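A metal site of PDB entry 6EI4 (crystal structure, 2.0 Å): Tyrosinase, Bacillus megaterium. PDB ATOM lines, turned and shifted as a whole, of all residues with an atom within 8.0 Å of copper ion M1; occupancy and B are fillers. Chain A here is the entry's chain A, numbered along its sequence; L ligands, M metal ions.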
ATOM      1  N   HIS A  39      19.927  -1.393   3.983  1.00  0.00           N
ATOM      2  CA  HIS A  39      20.687  -2.228   4.904  1.00  0.00           C
ATOM      3  C   HIS A  39      22.149  -2.301   4.496  1.00  0.00           C
ATOM      4  O   HIS A  39      23.046  -2.187   5.336  1.00  0.00           O
ATOM      5  CB  HIS A  39      20.075  -3.631   4.963  1.00  0.00           C
ATOM      6  CG  HIS A  39      20.655  -4.503   6.020  1.00  0.00           C
ATOM      7  ND1 HIS A  39      21.530  -5.536   5.752  1.00  0.00           N
ATOM      8  CD2 HIS A  39      20.488  -4.498   7.366  1.00  0.00           C
ATOM      9  CE1 HIS A  39      21.869  -6.126   6.880  1.00  0.00           C
ATOM     10  NE2 HIS A  39      21.254  -5.515   7.877  1.00  0.00           N
ATOM     11  N   ALA A  56      24.236   0.430  11.304  1.00  0.00           N
ATOM     12  CA  ALA A  56      23.236  -0.586  11.624  1.00  0.00           C
ATOM     13  C   ALA A  56      23.766  -1.760  12.462  1.00  0.00           C
ATOM     14  O   ALA A  56      22.974  -2.527  12.992  1.00  0.00           O
ATOM     15  CB  ALA A  56      22.624  -1.112  10.346  1.00  0.00           C
ATOM     16  N   HIS A  57      25.087  -1.893  12.581  1.00  0.00           N
ATOM     17  CA  HIS A  57      25.644  -3.063  13.266  1.00  0.00           C
ATOM     18  C   HIS A  57      26.903  -2.755  14.051  1.00  0.00           C
ATOM     19  O   HIS A  57      27.532  -1.707  13.874  1.00  0.00           O
ATOM     20  CB  HIS A  57      25.969  -4.171  12.260  1.00  0.00           C
ATOM     21  CG  HIS A  57      24.847  -4.483  11.310  1.00  0.00           C
ATOM     22  ND1 HIS A  57      24.712  -3.859  10.099  1.00  0.00           N
ATOM     23  CD2 HIS A  57      23.827  -5.364  11.404  1.00  0.00           C
ATOM     24  CE1 HIS A  57      23.648  -4.331   9.480  1.00  0.00           C
ATOM     25  NE2 HIS A  57      23.093  -5.247  10.252  1.00  0.00           N
ATOM     26  N   PHE A  62      22.439  -0.642  16.694  1.00  0.00           N
ATOM     27  CA  PHE A  62      22.011  -1.895  16.080  1.00  0.00           C
ATOM     28  C   PHE A  62      20.536  -2.200  16.308  1.00  0.00           C
ATOM     29  O   PHE A  62      19.807  -2.526  15.361  1.00  0.00           O
ATOM     30  CB  PHE A  62      22.858  -3.054  16.606  1.00  0.00           C
ATOM     31  CG  PHE A  62      22.286  -4.416  16.297  1.00  0.00           C
ATOM     32  CD1 PHE A  62      22.280  -4.908  15.001  1.00  0.00           C
ATOM     33  CD2 PHE A  62      21.756  -5.211  17.311  1.00  0.00           C
ATOM     34  CE1 PHE A  62      21.750  -6.158  14.719  1.00  0.00           C
ATOM     35  CE2 PHE A  62      21.230  -6.449  17.033  1.00  0.00           C
ATOM     36  CZ  PHE A  62      21.230  -6.934  15.734  1.00  0.00           C
ATOM     37  N   HIS A  66      17.294  -1.370  13.403  1.00  0.00           N
ATOM     38  CA  HIS A  66      16.497  -2.424  12.813  1.00  0.00           C
ATOM     39  C   HIS A  66      15.035  -2.310  13.216  1.00  0.00           C
ATOM     40  O   HIS A  66      14.167  -2.741  12.478  1.00  0.00           O
ATOM     41  CB  HIS A  66      17.053  -3.804  13.190  1.00  0.00           C
ATOM     42  CG  HIS A  66      18.344  -4.132  12.498  1.00  0.00           C
ATOM     43  ND1 HIS A  66      19.570  -3.692  12.972  1.00  0.00           N
ATOM     44  CD2 HIS A  66      18.606  -4.826  11.377  1.00  0.00           C
ATOM     45  CE1 HIS A  66      20.522  -4.122  12.178  1.00  0.00           C
ATOM     46  NE2 HIS A  66      19.963  -4.818  11.196  1.00  0.00           N
ATOM     47  N   GLU A 192      23.080  -8.861  19.916  1.00  0.00           N
ATOM     48  CA  GLU A 192      23.687  -8.804  18.588  1.00  0.00           C
ATOM     49  C   GLU A 192      24.418 -10.116  18.312  1.00  0.00           C
ATOM     50  O   GLU A 192      24.235 -10.724  17.257  1.00  0.00           O
ATOM     51  CB  GLU A 192      24.655  -7.629  18.467  1.00  0.00           C
ATOM     52  CG  GLU A 192      25.301  -7.516  17.086  1.00  0.00           C
ATOM     53  CD  GLU A 192      25.515  -6.092  16.635  1.00  0.00           C
ATOM     54  OE1 GLU A 192      25.683  -5.867  15.420  1.00  0.00           O
ATOM     55  OE2 GLU A 192      25.532  -5.197  17.507  1.00  0.00           O
ATOM     56  N   HIS A 201      21.488 -13.364  17.573  1.00  0.00           N
ATOM     57  CA  HIS A 201      21.237 -12.747  16.273  1.00  0.00           C
ATOM     58  C   HIS A 201      22.269 -13.125  15.203  1.00  0.00           C
ATOM     59  O   HIS A 201      21.906 -13.601  14.122  1.00  0.00           O
ATOM     60  CB  HIS A 201      21.185 -11.221  16.394  1.00  0.00           C
ATOM     61  CG  HIS A 201      21.353 -10.501  15.096  1.00  0.00           C
ATOM     62  ND1 HIS A 201      22.574 -10.035  14.651  1.00  0.00           N
ATOM     63  CD2 HIS A 201      20.463 -10.169  14.136  1.00  0.00           C
ATOM     64  CE1 HIS A 201      22.423  -9.452  13.478  1.00  0.00           C
ATOM     65  NE2 HIS A 201      21.147  -9.511  13.141  1.00  0.00           N
ATOM     66  N   ASN A 202      23.547 -12.886  15.493  1.00  0.00           N
ATOM     67  CA  ASN A 202      24.609 -13.218  14.549  1.00  0.00           C
ATOM     68  C   ASN A 202      24.634 -14.696  14.216  1.00  0.00           C
ATOM     69  O   ASN A 202      24.914 -15.075  13.070  1.00  0.00           O
ATOM     70  CB  ASN A 202      25.964 -12.797  15.112  1.00  0.00           C
ATOM     71  CG  ASN A 202      26.189 -11.294  15.067  1.00  0.00           C
ATOM     72  OD1 ASN A 202      25.452 -10.574  14.398  1.00  0.00           O
ATOM     73  ND2 ASN A 202      27.210 -10.824  15.762  1.00  0.00           N
ATOM     74  N   VAL A 204      22.064 -16.815  14.198  1.00  0.00           N
ATOM     75  CA  VAL A 204      20.942 -17.092  13.302  1.00  0.00           C
ATOM     76  C   VAL A 204      21.311 -16.877  11.835  1.00  0.00           C
ATOM     77  O   VAL A 204      21.096 -17.756  11.008  1.00  0.00           O
ATOM     78  CB  VAL A 204      19.721 -16.218  13.646  1.00  0.00           C
ATOM     79  CG1 VAL A 204      18.609 -16.462  12.634  1.00  0.00           C
ATOM     80  CG2 VAL A 204      19.232 -16.527  15.053  1.00  0.00           C
ATOM     81  N   HIS A 205      21.833 -15.691  11.526  1.00  0.00           N
ATOM     82  CA  HIS A 205      22.307 -15.373  10.187  1.00  0.00           C
ATOM     83  C   HIS A 205      23.260 -16.449   9.649  1.00  0.00           C
ATOM     84  O   HIS A 205      23.071 -16.967   8.547  1.00  0.00           O
ATOM     85  CB  HIS A 205      22.993 -14.010  10.167  1.00  0.00           C
ATOM     86  CG  HIS A 205      22.038 -12.854  10.137  1.00  0.00           C
ATOM     87  ND1 HIS A 205      21.219 -12.599   9.068  1.00  0.00           N
ATOM     88  CD2 HIS A 205      21.771 -11.900  11.062  1.00  0.00           C
ATOM     89  CE1 HIS A 205      20.473 -11.535   9.330  1.00  0.00           C
ATOM     90  NE2 HIS A 205      20.800 -11.080  10.532  1.00  0.00           N
ATOM     91  N   MET A 212      21.577 -14.750   3.742  1.00  0.00           N
ATOM     92  CA  MET A 212      21.420 -14.406   5.149  1.00  0.00           C
ATOM     93  C   MET A 212      22.759 -14.458   5.890  1.00  0.00           C
ATOM     94  O   MET A 212      22.911 -13.862   6.953  1.00  0.00           O
ATOM     95  CB  MET A 212      20.412 -15.339   5.834  1.00  0.00           C
ATOM     96  CG  MET A 212      18.972 -14.881   5.715  1.00  0.00           C
ATOM     97  SD  MET A 212      18.582 -13.505   6.818  1.00  0.00           S
ATOM     98  CE  MET A 212      18.344 -14.366   8.371  1.00  0.00           C
ATOM     99  N   VAL A 215      26.180  -9.784   5.613  1.00  0.00           N
ATOM    100  CA  VAL A 215      25.523  -8.513   5.928  1.00  0.00           C
ATOM    101  C   VAL A 215      24.867  -7.721   4.805  1.00  0.00           C
ATOM    102  O   VAL A 215      23.733  -7.265   4.965  1.00  0.00           O
ATOM    103  CB  VAL A 215      26.487  -7.570   6.683  1.00  0.00           C
ATOM    104  CG1 VAL A 215      25.703  -6.507   7.432  1.00  0.00           C
ATOM    105  CG2 VAL A 215      27.367  -8.367   7.629  1.00  0.00           C
ATOM    106  N   ALA A 218      21.762 -10.054   3.162  1.00  0.00           N
ATOM    107  CA  ALA A 218      20.822 -10.786   4.031  1.00  0.00           C
ATOM    108  C   ALA A 218      19.334 -10.467   3.796  1.00  0.00           C
ATOM    109  O   ALA A 218      18.511 -11.398   3.790  1.00  0.00           O
ATOM    110  CB  ALA A 218      21.176 -10.534   5.489  1.00  0.00           C
ATOM    111  N   PRO A 219      18.954  -9.189   3.596  1.00  0.00           N
ATOM    112  CA  PRO A 219      17.526  -8.932   3.384  1.00  0.00           C
ATOM    113  C   PRO A 219      16.938  -9.513   2.094  1.00  0.00           C
ATOM    114  O   PRO A 219      15.721  -9.440   1.922  1.00  0.00           O
ATOM    115  CB  PRO A 219      17.451  -7.402   3.341  1.00  0.00           C
ATOM    116  CG  PRO A 219      18.626  -6.957   4.128  1.00  0.00           C
ATOM    117  CD  PRO A 219      19.708  -7.932   3.772  1.00  0.00           C
ATOM    118  N   PHE A 224      14.559 -12.682   6.845  1.00  0.00           N
ATOM    119  CA  PHE A 224      15.383 -11.691   7.525  1.00  0.00           C
ATOM    120  C   PHE A 224      14.507 -10.829   8.418  1.00  0.00           C
ATOM    121  O   PHE A 224      14.894 -10.476   9.539  1.00  0.00           O
ATOM    122  CB  PHE A 224      16.132 -10.822   6.500  1.00  0.00           C
ATOM    123  CG  PHE A 224      16.828  -9.607   7.077  1.00  0.00           C
ATOM    124  CD1 PHE A 224      16.135  -8.437   7.335  1.00  0.00           C
ATOM    125  CD2 PHE A 224      18.187  -9.637   7.348  1.00  0.00           C
ATOM    126  CE1 PHE A 224      16.782  -7.326   7.850  1.00  0.00           C
ATOM    127  CE2 PHE A 224      18.834  -8.536   7.872  1.00  0.00           C
ATOM    128  CZ  PHE A 224      18.131  -7.375   8.118  1.00  0.00           C
ATOM    129  N   HIS A 227      13.118 -12.854  11.331  1.00  0.00           N
ATOM    130  CA  HIS A 227      14.239 -12.976  12.259  1.00  0.00           C
ATOM    131  C   HIS A 227      14.384 -11.729  13.140  1.00  0.00           C
ATOM    132  O   HIS A 227      14.401 -11.826  14.367  1.00  0.00           O
ATOM    133  CB  HIS A 227      15.524 -13.242  11.487  1.00  0.00           C
ATOM    134  CG  HIS A 227      16.780 -13.081  12.292  1.00  0.00           C
ATOM    135  ND1 HIS A 227      16.870 -13.469  13.607  1.00  0.00           N
ATOM    136  CD2 HIS A 227      17.991 -12.596  11.950  1.00  0.00           C
ATOM    137  CE1 HIS A 227      18.096 -13.208  14.062  1.00  0.00           C
ATOM    138  NE2 HIS A 227      18.795 -12.678  13.066  1.00  0.00           N
ATOM    139  N   HIS A 228      14.484 -10.563  12.503  1.00  0.00           N
ATOM    140  CA  HIS A 228      14.715  -9.345  13.258  1.00  0.00           C
ATOM    141  C   HIS A 228      13.497  -8.926  14.074  1.00  0.00           C
ATOM    142  O   HIS A 228      13.635  -8.226  15.075  1.00  0.00           O
ATOM    143  CB  HIS A 228      15.163  -8.216  12.322  1.00  0.00           C
ATOM    144  CG  HIS A 228      16.640  -8.175  12.115  1.00  0.00           C
ATOM    145  ND1 HIS A 228      17.509  -7.588  13.014  1.00  0.00           N
ATOM    146  CD2 HIS A 228      17.410  -8.688  11.126  1.00  0.00           C
ATOM    147  CE1 HIS A 228      18.748  -7.733  12.574  1.00  0.00           C
ATOM    148  NE2 HIS A 228      18.720  -8.387  11.437  1.00  0.00           N
ATOM    149  N   VAL A 231      14.124 -10.560  17.145  1.00  0.00           N
ATOM    150  CA  VAL A 231      15.180  -9.808  17.809  1.00  0.00           C
ATOM    151  C   VAL A 231      14.592  -8.565  18.464  1.00  0.00           C
ATOM    152  O   VAL A 231      14.933  -8.208  19.588  1.00  0.00           O
ATOM    153  CB  VAL A 231      16.289  -9.395  16.811  1.00  0.00           C
ATOM    154  CG1 VAL A 231      17.287  -8.459  17.478  1.00  0.00           C
ATOM    155  CG2 VAL A 231      16.990 -10.636  16.260  1.00  0.00           C
HETATM  156  C1  LIG L   1      24.677  -9.397  10.426  1.00  0.00           C
HETATM  157  C2  LIG L   1      23.574  -8.538  10.524  1.00  0.00           C
HETATM  158  C3  LIG L   1      24.870 -10.167   9.267  1.00  0.00           C
HETATM  159  C4  LIG L   1      22.679  -8.444   9.480  1.00  0.00           C
HETATM  160  C5  LIG L   1      23.965 -10.075   8.232  1.00  0.00           C
HETATM  161  C6  LIG L   1      22.868  -9.209   8.327  1.00  0.00           C
HETATM  162  C7  LIG L   1      26.081 -11.118   9.156  1.00  0.00           C
HETATM  163  C8  LIG L   1      27.831 -13.370   9.202  1.00  0.00           C
HETATM  164  C9  LIG L   1      26.298 -13.326   9.029  1.00  0.00           C
HETATM  165  C10 LIG L   1      27.280 -12.268  11.481  1.00  0.00           C
HETATM  166  C11 LIG L   1      25.825 -12.380  10.966  1.00  0.00           C
HETATM  167  C12 LIG L   1      29.534 -13.472  11.102  1.00  0.00           C
HETATM  168  C13 LIG L   1      29.944 -13.125  12.577  1.00  0.00           C
HETATM  169  C14 LIG L   1      31.559 -12.211  14.118  1.00  0.00           C
HETATM  170  C15 LIG L   1      31.192 -12.516  12.832  1.00  0.00           C
HETATM  171  C16 LIG L   1      30.678 -12.511  15.200  1.00  0.00           C
HETATM  172  C17 LIG L   1      29.450 -13.109  14.946  1.00  0.00           C
HETATM  173  C18 LIG L   1      29.083 -13.422  13.639  1.00  0.00           C
HETATM  174  C19 LIG L   1      32.129 -12.200  11.669  1.00  0.00           C
HETATM  175  F1  LIG L   1      21.589  -7.601   9.569  1.00  0.00           F
HETATM  176  N1  LIG L   1      25.749 -12.325   9.664  1.00  0.00           N
HETATM  177  N2  LIG L   1      28.202 -13.033  10.585  1.00  0.00           N
HETATM  178  O1  LIG L   1      30.280 -14.091  10.390  1.00  0.00           O
HETATM  179 CU    CU M   1      20.533  -9.227  11.313  1.00  0.00          CU
HETATM  180 CU    CU M   2      21.311  -5.732   9.815  1.00  0.00          CU
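Merely in contact with copper ion M1: Phe 224 (3.9 Å). Of the 18 residues printed, 4 come within 4 Å of copper ion M1.
O of His 201 sits close to NE2 of His 227, at 3.4 Å. The backbone carbonyl oxygen (O) of Glu 192 is in hydrogen-bond range of a ring nitrogen (ND1) of His 201. The backbone carbonyl oxygen (O) of Met 212 is in hydrogen-bond range of a ring nitrogen (ND1) of His 205 (3.0 Å). A ring nitrogen (ND1) of His 201 sits at hydrogen-bond distance from the side-chain amide oxygen (OD1) of Asn 202 (2.9 Å).
NE2 of His 201 binds copper ion M1 (1.9 Å). Copper ion M1 is bound by NE2 of His 228 (2.0 Å). Copper ion M1 is bound by NE2 of His 205. Slightly farther from copper ion M1 lies F1 of the ligand (2.6 Å).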
